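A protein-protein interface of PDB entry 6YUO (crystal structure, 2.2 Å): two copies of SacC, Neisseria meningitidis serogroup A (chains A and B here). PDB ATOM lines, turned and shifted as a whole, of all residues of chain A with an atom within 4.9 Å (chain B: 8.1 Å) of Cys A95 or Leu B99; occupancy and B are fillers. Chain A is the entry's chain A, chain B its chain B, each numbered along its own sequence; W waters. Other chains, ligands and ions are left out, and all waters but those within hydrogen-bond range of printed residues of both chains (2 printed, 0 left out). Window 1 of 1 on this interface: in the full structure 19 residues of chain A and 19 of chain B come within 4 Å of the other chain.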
ATOM      1  N   LEU A   2      19.066  25.384   7.664  1.00  0.00           N
ATOM      2  CA  LEU A   2      18.115  24.300   7.897  1.00  0.00           C
ATOM      3  C   LEU A   2      17.529  24.365   9.302  1.00  0.00           C
ATOM      4  O   LEU A   2      16.313  24.232   9.484  1.00  0.00           O
ATOM      5  CB  LEU A   2      18.788  22.947   7.657  1.00  0.00           C
ATOM      6  CG  LEU A   2      17.866  21.736   7.831  1.00  0.00           C
ATOM      7  CD1 LEU A   2      16.724  21.777   6.823  1.00  0.00           C
ATOM      8  CD2 LEU A   2      18.641  20.434   7.719  1.00  0.00           C
ATOM      9  N   LEU A   5      14.576  26.397   9.885  1.00  0.00           N
ATOM     10  CA  LEU A   5      13.343  25.947   9.253  1.00  0.00           C
ATOM     11  C   LEU A   5      12.511  25.047  10.155  1.00  0.00           C
ATOM     12  O   LEU A   5      11.441  24.594   9.734  1.00  0.00           O
ATOM     13  CB  LEU A   5      13.661  25.209   7.947  1.00  0.00           C
ATOM     14  CG  LEU A   5      14.491  25.954   6.902  1.00  0.00           C
ATOM     15  CD1 LEU A   5      14.798  25.036   5.734  1.00  0.00           C
ATOM     16  CD2 LEU A   5      13.771  27.202   6.420  1.00  0.00           C
ATOM     17  N   LEU A  19       9.785  24.531   4.434  1.00  0.00           N
ATOM     18  CA  LEU A  19      10.364  25.449   3.457  1.00  0.00           C
ATOM     19  C   LEU A  19       9.340  25.672   2.356  1.00  0.00           C
ATOM     20  O   LEU A  19       8.918  24.714   1.698  1.00  0.00           O
ATOM     21  CB  LEU A  19      11.670  24.891   2.880  1.00  0.00           C
ATOM     22  CG  LEU A  19      12.394  25.726   1.814  1.00  0.00           C
ATOM     23  CD1 LEU A  19      12.874  27.059   2.368  1.00  0.00           C
ATOM     24  CD2 LEU A  19      13.559  24.945   1.209  1.00  0.00           C
ATOM     25  N   GLN A  91       8.653  21.334  -7.095  1.00  0.00           N
ATOM     26  CA  GLN A  91       9.909  22.064  -7.217  1.00  0.00           C
ATOM     27  C   GLN A  91      10.623  22.152  -5.876  1.00  0.00           C
ATOM     28  O   GLN A  91      11.829  21.891  -5.780  1.00  0.00           O
ATOM     29  CB  GLN A  91       9.629  23.463  -7.752  1.00  0.00           C
ATOM     30  CG  GLN A  91      10.298  23.804  -9.046  1.00  0.00           C
ATOM     31  CD  GLN A  91      10.106  25.267  -9.403  1.00  0.00           C
ATOM     32  OE1 GLN A  91       9.268  25.603 -10.241  1.00  0.00           O
ATOM     33  NE2 GLN A  91      10.876  26.146  -8.763  1.00  0.00           N
ATOM     34  N   THR A  92       9.889  22.538  -4.829  1.00  0.00           N
ATOM     35  CA  THR A  92      10.475  22.677  -3.500  1.00  0.00           C
ATOM     36  C   THR A  92      10.947  21.332  -2.965  1.00  0.00           C
ATOM     37  O   THR A  92      12.051  21.218  -2.421  1.00  0.00           O
ATOM     38  CB  THR A  92       9.458  23.308  -2.549  1.00  0.00           C
ATOM     39  OG1 THR A  92       9.022  24.560  -3.092  1.00  0.00           O
ATOM     40  CG2 THR A  92      10.080  23.545  -1.182  1.00  0.00           C
ATOM     41  N   ILE A  93      10.116  20.296  -3.115  1.00  0.00           N
ATOM     42  CA  ILE A  93      10.508  18.949  -2.702  1.00  0.00           C
ATOM     43  C   ILE A  93      11.798  18.535  -3.399  1.00  0.00           C
ATOM     44  O   ILE A  93      12.729  18.020  -2.768  1.00  0.00           O
ATOM     45  CB  ILE A  93       9.371  17.955  -2.983  1.00  0.00           C
ATOM     46  CG1 ILE A  93       8.181  18.239  -2.072  1.00  0.00           C
ATOM     47  CG2 ILE A  93       9.851  16.517  -2.814  1.00  0.00           C
ATOM     48  CD1 ILE A  93       6.996  17.345  -2.330  1.00  0.00           C
ATOM     49  N   HIS A  94      11.866  18.748  -4.715  1.00  0.00           N
ATOM     50  CA  HIS A  94      13.053  18.370  -5.474  1.00  0.00           C
ATOM     51  C   HIS A  94      14.291  19.082  -4.948  1.00  0.00           C
ATOM     52  O   HIS A  94      15.352  18.470  -4.773  1.00  0.00           O
ATOM     53  CB  HIS A  94      12.843  18.685  -6.957  1.00  0.00           C
ATOM     54  CG  HIS A  94      14.009  18.334  -7.823  1.00  0.00           C
ATOM     55  ND1 HIS A  94      14.534  17.061  -7.884  1.00  0.00           N
ATOM     56  CD2 HIS A  94      14.749  19.088  -8.670  1.00  0.00           C
ATOM     57  CE1 HIS A  94      15.546  17.045  -8.732  1.00  0.00           C
ATOM     58  NE2 HIS A  94      15.700  18.262  -9.221  1.00  0.00           N
ATOM     59  N   CYS A  95      14.165  20.384  -4.681  1.00  0.00           N
ATOM     60  CA  CYS A  95      15.285  21.149  -4.147  1.00  0.00           C
ATOM     61  C   CYS A  95      15.717  20.621  -2.785  1.00  0.00           C
ATOM     62  O   CYS A  95      16.916  20.529  -2.499  1.00  0.00           O
ATOM     63  CB  CYS A  95      14.910  22.630  -4.060  1.00  0.00           C
ATOM     64  SG  CYS A  95      14.822  23.485  -5.646  1.00  0.00           S
ATOM     65  N   ILE A  96      14.756  20.244  -1.943  1.00  0.00           N
ATOM     66  CA  ILE A  96      15.083  19.736  -0.612  1.00  0.00           C
ATOM     67  C   ILE A  96      15.837  18.421  -0.717  1.00  0.00           C
ATOM     68  O   ILE A  96      16.851  18.206  -0.042  1.00  0.00           O
ATOM     69  CB  ILE A  96      13.805  19.592   0.230  1.00  0.00           C
ATOM     70  CG1 ILE A  96      13.306  20.975   0.636  1.00  0.00           C
ATOM     71  CG2 ILE A  96      14.052  18.705   1.442  1.00  0.00           C
ATOM     72  CD1 ILE A  96      11.824  21.034   0.895  1.00  0.00           C
ATOM     73  N   ILE A  97      15.358  17.523  -1.575  1.00  0.00           N
ATOM     74  CA  ILE A  97      16.005  16.225  -1.727  1.00  0.00           C
ATOM     75  C   ILE A  97      17.407  16.393  -2.293  1.00  0.00           C
ATOM     76  O   ILE A  97      18.379  15.852  -1.757  1.00  0.00           O
ATOM     77  CB  ILE A  97      15.152  15.300  -2.608  1.00  0.00           C
ATOM     78  CG1 ILE A  97      13.827  15.008  -1.913  1.00  0.00           C
ATOM     79  CG2 ILE A  97      15.904  14.014  -2.921  1.00  0.00           C
ATOM     80  CD1 ILE A  97      12.892  14.192  -2.757  1.00  0.00           C
ATOM     81  N   GLN A  98      17.534  17.173  -3.371  1.00  0.00           N
ATOM     82  CA  GLN A  98      18.812  17.271  -4.071  1.00  0.00           C
ATOM     83  C   GLN A  98      19.905  17.853  -3.185  1.00  0.00           C
ATOM     84  O   GLN A  98      21.071  17.456  -3.290  1.00  0.00           O
ATOM     85  CB  GLN A  98      18.655  18.110  -5.339  1.00  0.00           C
ATOM     86  CG  GLN A  98      17.943  17.378  -6.455  1.00  0.00           C
ATOM     87  CD  GLN A  98      18.586  16.040  -6.757  1.00  0.00           C
ATOM     88  OE1 GLN A  98      19.764  15.970  -7.100  1.00  0.00           O
ATOM     89  NE2 GLN A  98      17.819  14.968  -6.610  1.00  0.00           N
ATOM     90  N   LEU A  99      19.558  18.795  -2.314  1.00  0.00           N
ATOM     91  CA  LEU A  99      20.566  19.472  -1.507  1.00  0.00           C
ATOM     92  C   LEU A  99      20.783  18.826  -0.146  1.00  0.00           C
ATOM     93  O   LEU A  99      21.847  19.027   0.451  1.00  0.00           O
ATOM     94  CB  LEU A  99      20.195  20.948  -1.327  1.00  0.00           C
ATOM     95  CG  LEU A  99      20.202  21.754  -2.629  1.00  0.00           C
ATOM     96  CD1 LEU A  99      19.830  23.201  -2.373  1.00  0.00           C
ATOM     97  CD2 LEU A  99      21.566  21.653  -3.304  1.00  0.00           C
ATOM     98  N   LEU A 100      19.822  18.054   0.358  1.00  0.00           N
ATOM     99  CA  LEU A 100      20.011  17.347   1.618  1.00  0.00           C
ATOM    100  C   LEU A 100      20.433  15.895   1.438  1.00  0.00           C
ATOM    101  O   LEU A 100      20.950  15.299   2.390  1.00  0.00           O
ATOM    102  CB  LEU A 100      18.733  17.400   2.463  1.00  0.00           C
ATOM    103  CG  LEU A 100      18.353  18.805   2.934  1.00  0.00           C
ATOM    104  CD1 LEU A 100      17.177  18.767   3.897  1.00  0.00           C
ATOM    105  CD2 LEU A 100      19.548  19.508   3.565  1.00  0.00           C
ATOM    106  N   MET B   1      21.917  14.981  -4.681  1.00  0.00           N
ATOM    107  CA  MET B   1      23.192  15.270  -4.036  1.00  0.00           C
ATOM    108  C   MET B   1      23.890  16.416  -4.752  1.00  0.00           C
ATOM    109  O   MET B   1      24.010  16.410  -5.981  1.00  0.00           O
ATOM    110  CB  MET B   1      24.085  14.028  -4.008  1.00  0.00           C
ATOM    111  CG  MET B   1      25.387  14.217  -3.241  1.00  0.00           C
ATOM    112  SD  MET B   1      26.197  12.657  -2.819  1.00  0.00           S
ATOM    113  CE  MET B   1      26.752  12.083  -4.424  1.00  0.00           C
ATOM    114  N   LEU B   5      24.914  17.821  -9.137  1.00  0.00           N
ATOM    115  CA  LEU B   5      24.342  18.959  -9.843  1.00  0.00           C
ATOM    116  C   LEU B   5      25.375  19.733 -10.652  1.00  0.00           C
ATOM    117  O   LEU B   5      25.013  20.724 -11.296  1.00  0.00           O
ATOM    118  CB  LEU B   5      23.664  19.915  -8.853  1.00  0.00           C
ATOM    119  CG  LEU B   5      22.603  19.331  -7.918  1.00  0.00           C
ATOM    120  CD1 LEU B   5      22.177  20.356  -6.874  1.00  0.00           C
ATOM    121  CD2 LEU B   5      21.403  18.845  -8.714  1.00  0.00           C
ATOM    122  N   LEU B  19      20.563  23.572 -10.534  1.00  0.00           N
ATOM    123  CA  LEU B  19      19.404  22.939  -9.923  1.00  0.00           C
ATOM    124  C   LEU B  19      18.157  23.575 -10.510  1.00  0.00           C
ATOM    125  O   LEU B  19      17.930  24.776 -10.326  1.00  0.00           O
ATOM    126  CB  LEU B  19      19.430  23.093  -8.399  1.00  0.00           C
ATOM    127  CG  LEU B  19      18.262  22.499  -7.611  1.00  0.00           C
ATOM    128  CD1 LEU B  19      18.073  21.027  -7.945  1.00  0.00           C
ATOM    129  CD2 LEU B  19      18.490  22.680  -6.119  1.00  0.00           C
ATOM    130  N   ASN B  20      17.371  22.774 -11.236  1.00  0.00           N
ATOM    131  CA  ASN B  20      16.085  23.202 -11.784  1.00  0.00           C
ATOM    132  C   ASN B  20      16.249  24.453 -12.647  1.00  0.00           C
ATOM    133  O   ASN B  20      15.466  25.403 -12.569  1.00  0.00           O
ATOM    134  CB  ASN B  20      15.072  23.420 -10.658  1.00  0.00           C
ATOM    135  CG  ASN B  20      13.655  23.573 -11.160  1.00  0.00           C
ATOM    136  OD1 ASN B  20      12.889  24.390 -10.646  1.00  0.00           O
ATOM    137  ND2 ASN B  20      13.293  22.786 -12.162  1.00  0.00           N
ATOM    138  N   CYS B  22      18.721  26.632 -12.494  1.00  0.00           N
ATOM    139  CA  CYS B  22      19.386  27.729 -11.796  1.00  0.00           C
ATOM    140  C   CYS B  22      20.858  27.389 -11.590  1.00  0.00           C
ATOM    141  O   CYS B  22      21.185  26.450 -10.859  1.00  0.00           O
ATOM    142  CB  CYS B  22      18.705  28.007 -10.456  1.00  0.00           C
ATOM    143  SG  CYS B  22      19.495  29.288  -9.448  1.00  0.00           S
ATOM    144  N   TYR B  26      28.986  27.935  -5.089  1.00  0.00           N
ATOM    145  CA  TYR B  26      28.792  27.777  -3.652  1.00  0.00           C
ATOM    146  C   TYR B  26      30.134  27.489  -2.996  1.00  0.00           C
ATOM    147  O   TYR B  26      30.791  26.497  -3.327  1.00  0.00           O
ATOM    148  CB  TYR B  26      27.785  26.657  -3.354  1.00  0.00           C
ATOM    149  CG  TYR B  26      27.654  26.292  -1.887  1.00  0.00           C
ATOM    150  CD1 TYR B  26      27.340  27.254  -0.934  1.00  0.00           C
ATOM    151  CD2 TYR B  26      27.830  24.980  -1.459  1.00  0.00           C
ATOM    152  CE1 TYR B  26      27.216  26.920   0.405  1.00  0.00           C
ATOM    153  CE2 TYR B  26      27.707  24.638  -0.120  1.00  0.00           C
ATOM    154  CZ  TYR B  26      27.399  25.612   0.805  1.00  0.00           C
ATOM    155  OH  TYR B  26      27.274  25.278   2.134  1.00  0.00           O
ATOM    156  N   LYS B  28      31.416  27.224   0.972  1.00  0.00           N
ATOM    157  CA  LYS B  28      30.960  27.221   2.355  1.00  0.00           C
ATOM    158  C   LYS B  28      31.985  27.913   3.244  1.00  0.00           C
ATOM    159  O   LYS B  28      33.181  27.612   3.177  1.00  0.00           O
ATOM    160  CB  LYS B  28      30.711  25.792   2.830  1.00  0.00           C
ATOM    161  CG  LYS B  28      30.219  25.685   4.265  1.00  0.00           C
ATOM    162  CD  LYS B  28      29.398  24.422   4.450  1.00  0.00           C
ATOM    163  CE  LYS B  28      29.209  24.086   5.915  1.00  0.00           C
ATOM    164  NZ  LYS B  28      29.001  22.622   6.101  1.00  0.00           N
ATOM    165  N   LEU B  63      27.465  32.478  -2.289  1.00  0.00           N
ATOM    166  CA  LEU B  63      26.608  31.948  -3.339  1.00  0.00           C
ATOM    167  C   LEU B  63      26.466  33.011  -4.417  1.00  0.00           C
ATOM    168  O   LEU B  63      26.131  34.159  -4.113  1.00  0.00           O
ATOM    169  CB  LEU B  63      25.229  31.557  -2.795  1.00  0.00           C
ATOM    170  CG  LEU B  63      25.106  30.265  -1.982  1.00  0.00           C
ATOM    171  CD1 LEU B  63      23.870  30.309  -1.093  1.00  0.00           C
ATOM    172  CD2 LEU B  63      25.047  29.058  -2.902  1.00  0.00           C
ATOM    173  N   GLY B  88       8.909  31.270  -9.949  1.00  0.00           N
ATOM    174  CA  GLY B  88       9.482  29.932  -9.870  1.00  0.00           C
ATOM    175  C   GLY B  88      10.995  29.915  -9.796  1.00  0.00           C
ATOM    176  O   GLY B  88      11.579  29.034  -9.158  1.00  0.00           O
ATOM    177  N   TYR B  89      11.651  30.888 -10.431  1.00  0.00           N
ATOM    178  CA  TYR B  89      13.107  30.960 -10.402  1.00  0.00           C
ATOM    179  C   TYR B  89      13.598  31.558  -9.089  1.00  0.00           C
ATOM    180  O   TYR B  89      14.524  31.028  -8.466  1.00  0.00           O
ATOM    181  CB  TYR B  89      13.613  31.769 -11.598  1.00  0.00           C
ATOM    182  CG  TYR B  89      15.081  31.577 -11.905  1.00  0.00           C
ATOM    183  CD1 TYR B  89      15.536  30.404 -12.499  1.00  0.00           C
ATOM    184  CD2 TYR B  89      16.010  32.569 -11.614  1.00  0.00           C
ATOM    185  CE1 TYR B  89      16.875  30.224 -12.787  1.00  0.00           C
ATOM    186  CE2 TYR B  89      17.351  32.400 -11.897  1.00  0.00           C
ATOM    187  CZ  TYR B  89      17.778  31.227 -12.484  1.00  0.00           C
ATOM    188  OH  TYR B  89      19.113  31.047 -12.770  1.00  0.00           O
ATOM    189  N   GLN B  91      12.013  31.388  -6.354  1.00  0.00           N
ATOM    190  CA  GLN B  91      11.745  30.345  -5.367  1.00  0.00           C
ATOM    191  C   GLN B  91      12.859  29.309  -5.333  1.00  0.00           C
ATOM    192  O   GLN B  91      13.240  28.828  -4.258  1.00  0.00           O
ATOM    193  CB  GLN B  91      10.407  29.676  -5.677  1.00  0.00           C
ATOM    194  CG  GLN B  91      10.070  28.510  -4.765  1.00  0.00           C
ATOM    195  CD  GLN B  91       8.791  27.805  -5.178  1.00  0.00           C
ATOM    196  OE1 GLN B  91       7.714  28.401  -5.168  1.00  0.00           O
ATOM    197  NE2 GLN B  91       8.905  26.533  -5.554  1.00  0.00           N
ATOM    198  N   THR B  92      13.385  28.944  -6.503  1.00  0.00           N
ATOM    199  CA  THR B  92      14.495  27.999  -6.551  1.00  0.00           C
ATOM    200  C   THR B  92      15.733  28.576  -5.874  1.00  0.00           C
ATOM    201  O   THR B  92      16.415  27.887  -5.106  1.00  0.00           O
ATOM    202  CB  THR B  92      14.797  27.622  -8.001  1.00  0.00           C
ATOM    203  OG1 THR B  92      13.668  26.957  -8.575  1.00  0.00           O
ATOM    204  CG2 THR B  92      16.004  26.710  -8.060  1.00  0.00           C
ATOM    205  N   ILE B  93      16.039  29.844  -6.155  1.00  0.00           N
ATOM    206  CA  ILE B  93      17.157  30.520  -5.499  1.00  0.00           C
ATOM    207  C   ILE B  93      16.960  30.520  -3.988  1.00  0.00           C
ATOM    208  O   ILE B  93      17.885  30.226  -3.221  1.00  0.00           O
ATOM    209  CB  ILE B  93      17.314  31.951  -6.049  1.00  0.00           C
ATOM    210  CG1 ILE B  93      17.798  31.925  -7.504  1.00  0.00           C
ATOM    211  CG2 ILE B  93      18.239  32.786  -5.163  1.00  0.00           C
ATOM    212  CD1 ILE B  93      17.597  33.242  -8.232  1.00  0.00           C
ATOM    213  N   HIS B  94      15.742  30.834  -3.546  1.00  0.00           N
ATOM    214  CA  HIS B  94      15.443  30.874  -2.116  1.00  0.00           C
ATOM    215  C   HIS B  94      15.696  29.520  -1.461  1.00  0.00           C
ATOM    216  O   HIS B  94      16.306  29.442  -0.388  1.00  0.00           O
ATOM    217  CB  HIS B  94      13.993  31.321  -1.910  1.00  0.00           C
ATOM    218  CG  HIS B  94      13.554  31.319  -0.480  1.00  0.00           C
ATOM    219  ND1 HIS B  94      14.186  32.059   0.492  1.00  0.00           N
ATOM    220  CD2 HIS B  94      12.539  30.672   0.139  1.00  0.00           C
ATOM    221  CE1 HIS B  94      13.580  31.868   1.651  1.00  0.00           C
ATOM    222  NE2 HIS B  94      12.578  31.029   1.465  1.00  0.00           N
ATOM    223  N   CYS B  95      15.245  28.439  -2.104  1.00  0.00           N
ATOM    224  CA  CYS B  95      15.464  27.101  -1.562  1.00  0.00           C
ATOM    225  C   CYS B  95      16.953  26.793  -1.442  1.00  0.00           C
ATOM    226  O   CYS B  95      17.410  26.267  -0.421  1.00  0.00           O
ATOM    227  CB  CYS B  95      14.766  26.059  -2.440  1.00  0.00           C
ATOM    228  SG  CYS B  95      12.956  26.100  -2.421  1.00  0.00           S
ATOM    229  N   ILE B  96      17.730  27.135  -2.472  1.00  0.00           N
ATOM    230  CA  ILE B  96      19.170  26.875  -2.453  1.00  0.00           C
ATOM    231  C   ILE B  96      19.841  27.628  -1.311  1.00  0.00           C
ATOM    232  O   ILE B  96      20.695  27.081  -0.602  1.00  0.00           O
ATOM    233  CB  ILE B  96      19.789  27.238  -3.818  1.00  0.00           C
ATOM    234  CG1 ILE B  96      19.311  26.253  -4.887  1.00  0.00           C
ATOM    235  CG2 ILE B  96      21.312  27.267  -3.747  1.00  0.00           C
ATOM    236  CD1 ILE B  96      19.479  26.757  -6.300  1.00  0.00           C
ATOM    237  N   ILE B  97      19.464  28.892  -1.111  1.00  0.00           N
ATOM    238  CA  ILE B  97      20.053  29.676  -0.033  1.00  0.00           C
ATOM    239  C   ILE B  97      19.664  29.105   1.324  1.00  0.00           C
ATOM    240  O   ILE B  97      20.516  28.904   2.195  1.00  0.00           O
ATOM    241  CB  ILE B  97      19.644  31.151  -0.162  1.00  0.00           C
ATOM    242  CG1 ILE B  97      20.178  31.731  -1.466  1.00  0.00           C
ATOM    243  CG2 ILE B  97      20.151  31.942   1.027  1.00  0.00           C
ATOM    244  CD1 ILE B  97      19.570  33.055  -1.818  1.00  0.00           C
ATOM    245  N   GLN B  98      18.378  28.824   1.527  1.00  0.00           N
ATOM    246  CA  GLN B  98      17.927  28.339   2.826  1.00  0.00           C
ATOM    247  C   GLN B  98      18.514  26.980   3.191  1.00  0.00           C
ATOM    248  O   GLN B  98      18.609  26.662   4.381  1.00  0.00           O
ATOM    249  CB  GLN B  98      16.404  28.277   2.857  1.00  0.00           C
ATOM    250  CG  GLN B  98      15.761  29.644   2.889  1.00  0.00           C
ATOM    251  CD  GLN B  98      16.320  30.504   4.000  1.00  0.00           C
ATOM    252  OE1 GLN B  98      16.258  30.135   5.172  1.00  0.00           O
ATOM    253  NE2 GLN B  98      16.883  31.651   3.637  1.00  0.00           N
ATOM    254  N   LEU B  99      18.912  26.174   2.209  1.00  0.00           N
ATOM    255  CA  LEU B  99      19.456  24.851   2.485  1.00  0.00           C
ATOM    256  C   LEU B  99      20.975  24.805   2.510  1.00  0.00           C
ATOM    257  O   LEU B  99      21.543  23.979   3.231  1.00  0.00           O
ATOM    258  CB  LEU B  99      18.935  23.844   1.456  1.00  0.00           C
ATOM    259  CG  LEU B  99      17.442  23.550   1.633  1.00  0.00           C
ATOM    260  CD1 LEU B  99      16.831  22.934   0.378  1.00  0.00           C
ATOM    261  CD2 LEU B  99      17.208  22.659   2.846  1.00  0.00           C
ATOM    262  N   LEU B 100      21.652  25.666   1.752  1.00  0.00           N
ATOM    263  CA  LEU B 100      23.108  25.669   1.736  1.00  0.00           C
ATOM    264  C   LEU B 100      23.728  26.707   2.666  1.00  0.00           C
ATOM    265  O   LEU B 100      24.916  26.596   2.983  1.00  0.00           O
ATOM    266  CB  LEU B 100      23.621  25.893   0.310  1.00  0.00           C
ATOM    267  CG  LEU B 100      23.300  24.772  -0.683  1.00  0.00           C
ATOM    268  CD1 LEU B 100      24.079  24.954  -1.980  1.00  0.00           C
ATOM    269  CD2 LEU B 100      23.572  23.400  -0.071  1.00  0.00           C
ATOM    270  N   SER B 101      22.968  27.706   3.109  1.00  0.00           N
ATOM    271  CA  SER B 101      23.513  28.718   4.001  1.00  0.00           C
ATOM    272  C   SER B 101      23.546  28.209   5.437  1.00  0.00           C
ATOM    273  O   SER B 101      22.687  27.432   5.866  1.00  0.00           O
ATOM    274  CB  SER B 101      22.695  30.006   3.924  1.00  0.00           C
ATOM    275  OG  SER B 101      23.288  31.044   4.680  1.00  0.00           O
ATOM    276  N   ASN B 102      24.558  28.655   6.183  1.00  0.00           N
ATOM    277  CA  ASN B 102      24.723  28.283   7.584  1.00  0.00           C
ATOM    278  C   ASN B 102      24.701  29.505   8.497  1.00  0.00           C
ATOM    279  O   ASN B 102      25.286  29.488   9.581  1.00  0.00           O
ATOM    280  CB  ASN B 102      26.004  27.472   7.789  1.00  0.00           C
ATOM    281  CG  ASN B 102      27.258  28.223   7.373  1.00  0.00           C
ATOM    282  OD1 ASN B 102      27.189  29.283   6.750  1.00  0.00           O
ATOM    283  ND2 ASN B 102      28.417  27.668   7.715  1.00  0.00           N
ATOM    284  N   TYR B 129      14.682  38.847   2.837  1.00  0.00           N
ATOM    285  CA  TYR B 129      16.105  39.023   3.097  1.00  0.00           C
ATOM    286  C   TYR B 129      16.337  40.504   3.372  1.00  0.00           C
ATOM    287  O   TYR B 129      16.223  41.319   2.444  1.00  0.00           O
ATOM    288  CB  TYR B 129      16.944  38.557   1.915  1.00  0.00           C
ATOM    289  CG  TYR B 129      16.911  37.063   1.662  1.00  0.00           C
ATOM    290  CD1 TYR B 129      15.855  36.477   0.971  1.00  0.00           C
ATOM    291  CD2 TYR B 129      17.938  36.238   2.102  1.00  0.00           C
ATOM    292  CE1 TYR B 129      15.822  35.115   0.734  1.00  0.00           C
ATOM    293  CE2 TYR B 129      17.915  34.870   1.869  1.00  0.00           C
ATOM    294  CZ  TYR B 129      16.851  34.317   1.183  1.00  0.00           C
ATOM    295  OH  TYR B 129      16.812  32.962   0.944  1.00  0.00           O
HETATM  296  O   HOH W   1      21.172  24.524   6.225  1.00  0.00           O
HETATM  297  O   HOH W   2      17.290  19.610 -11.700  1.00  0.00           O
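The side-chain amide oxygen (OD1) of Asn B20 sits close to the side-chain amide nitrogen (NE2) of Gln A91 (3.3 Å). The backbone carbonyl oxygen (O) of Gly B88 sits at hydrogen-bond distance from the side-chain amide nitrogen (NE2) of Gln A91 (3.0 Å). The side-chain amide nitrogen of Gln A91 lies within hydrogen-bond range of the side-chain hydroxyl of Thr B92 (2.9 Å). The side-chain amide nitrogen of Gln B91 is in hydrogen-bond range of the side-chain hydroxyl of Thr A92 (3.2 Å). O of Gln A98 lies within hydrogen-bond range of N of Met B1 (3.0 Å).
O of Gln A91 is in hydrogen-bond range of SG of Cys A95. OD1 of Asn B20 sits at hydrogen-bond distance from OG1 of Thr B92, at 3.4 Å. The backbone carbonyl oxygen of Gly B88 sits at hydrogen-bond distance from the side-chain hydroxyl of Thr B92, at 3.0 Å. The backbone carbonyl oxygen of Gln B91 lies within hydrogen-bond range of the side-chain sulfur of Cys B95. The side-chain hydroxyl (OH) of Tyr B129 lies within hydrogen-bond range of the side-chain amide nitrogen (NE2) of Gln B98.
Gln B98 touches Leu A2. Gln B98 touches Leu A19 (CB to CD1, 3.8 Å). Gln A91 touches Gln B91 (NE2 to NE2, 3.8 Å). His A94 touches Leu B19 (NE2 to CD1, 3.9 Å). CD1 of Leu B99 touches O of Cys A95, at 3.8 Å. Ile A96 touches Leu B99. Gln A98 touches Leu B5. CD2 of Leu B19 touches CG of Leu A99 (3.996 Å). CD1 of Leu A99 touches CA of Ile B96 (3.7 Å). Leu A99 touches Leu B99.
Cys A95 touches three residues of chain B. Printed residues of chain A within 4 Å of Leu B19: His A94 (3.9 Å), Cys A95 (3.8 Å), Gln A98 (3.9 Å) and Leu A99 (3.996 Å). Printed residues of chain A within 4 Å of Gly B88: Gln A91 (3.0 Å). Of the printed residues of chain B, Ile A96 touches Leu B99. Of the printed residues of chain B, Leu A100 touches Leu B99. Printed residues of chain A within 4 Å of Cys B95: Leu A19 (3.9 Å) and Cys A95 (3.8 Å). The nearest printed residue of chain A that does not touch Leu B99 is Leu A2 (4.1 Å).
Printed residues of chain A that touch a printed residue of chain B: Leu A2, Leu A19, Gln A91, Thr A92, His A94, Cys A95, Ile A96, Gln A98, Leu A99 and Leu A100. Hydrophobic or aromatic side chains of chain A that line the printed part of chain B: Leu A19, His A94, Leu A99 and Leu A100. Of the 23 printed residues of chain B, 11 touch a printed residue of chain A. Printed residues of chain B that touch a printed residue of chain A: Met B1, Leu B5, Leu B19, Asn B20, Gly B88, Gln B91, Thr B92, Cys B95, Ile B96, Gln B98 and Leu B99. Hydrophobic or aromatic side chains of chain B within 4 Å of the printed part of chain A: Leu B5, Leu B19, Ile B96 and Leu B99.
Leu A19 touches Leu B99, and with the chains exchanged Leu A99 touches Leu B19. Gln A91 touches its own counterpart, Gln B91. Cys B95 touches its own counterpart, Cys A95. Leu A99 touches Leu B5, but with the chains exchanged Leu A5 does not touch Leu B99 (4.4 Å). Positions printed for both chains: 5, 19, 91, 92, 93, 94, 95, 96, 97, 98, 99 and 100.
Water W1 lies within hydrogen-bond range of the backbone NH (N) of Leu A2 (2.7 Å), the backbone carbonyl oxygen (O) of Leu B99 (3.1 Å) and the backbone carbonyl oxygen (O) of Ser B101 (3.3 Å). Water W2 bridges N of Asn B20 (3.2 Å) and NE2 of His A94 (3.2 Å).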
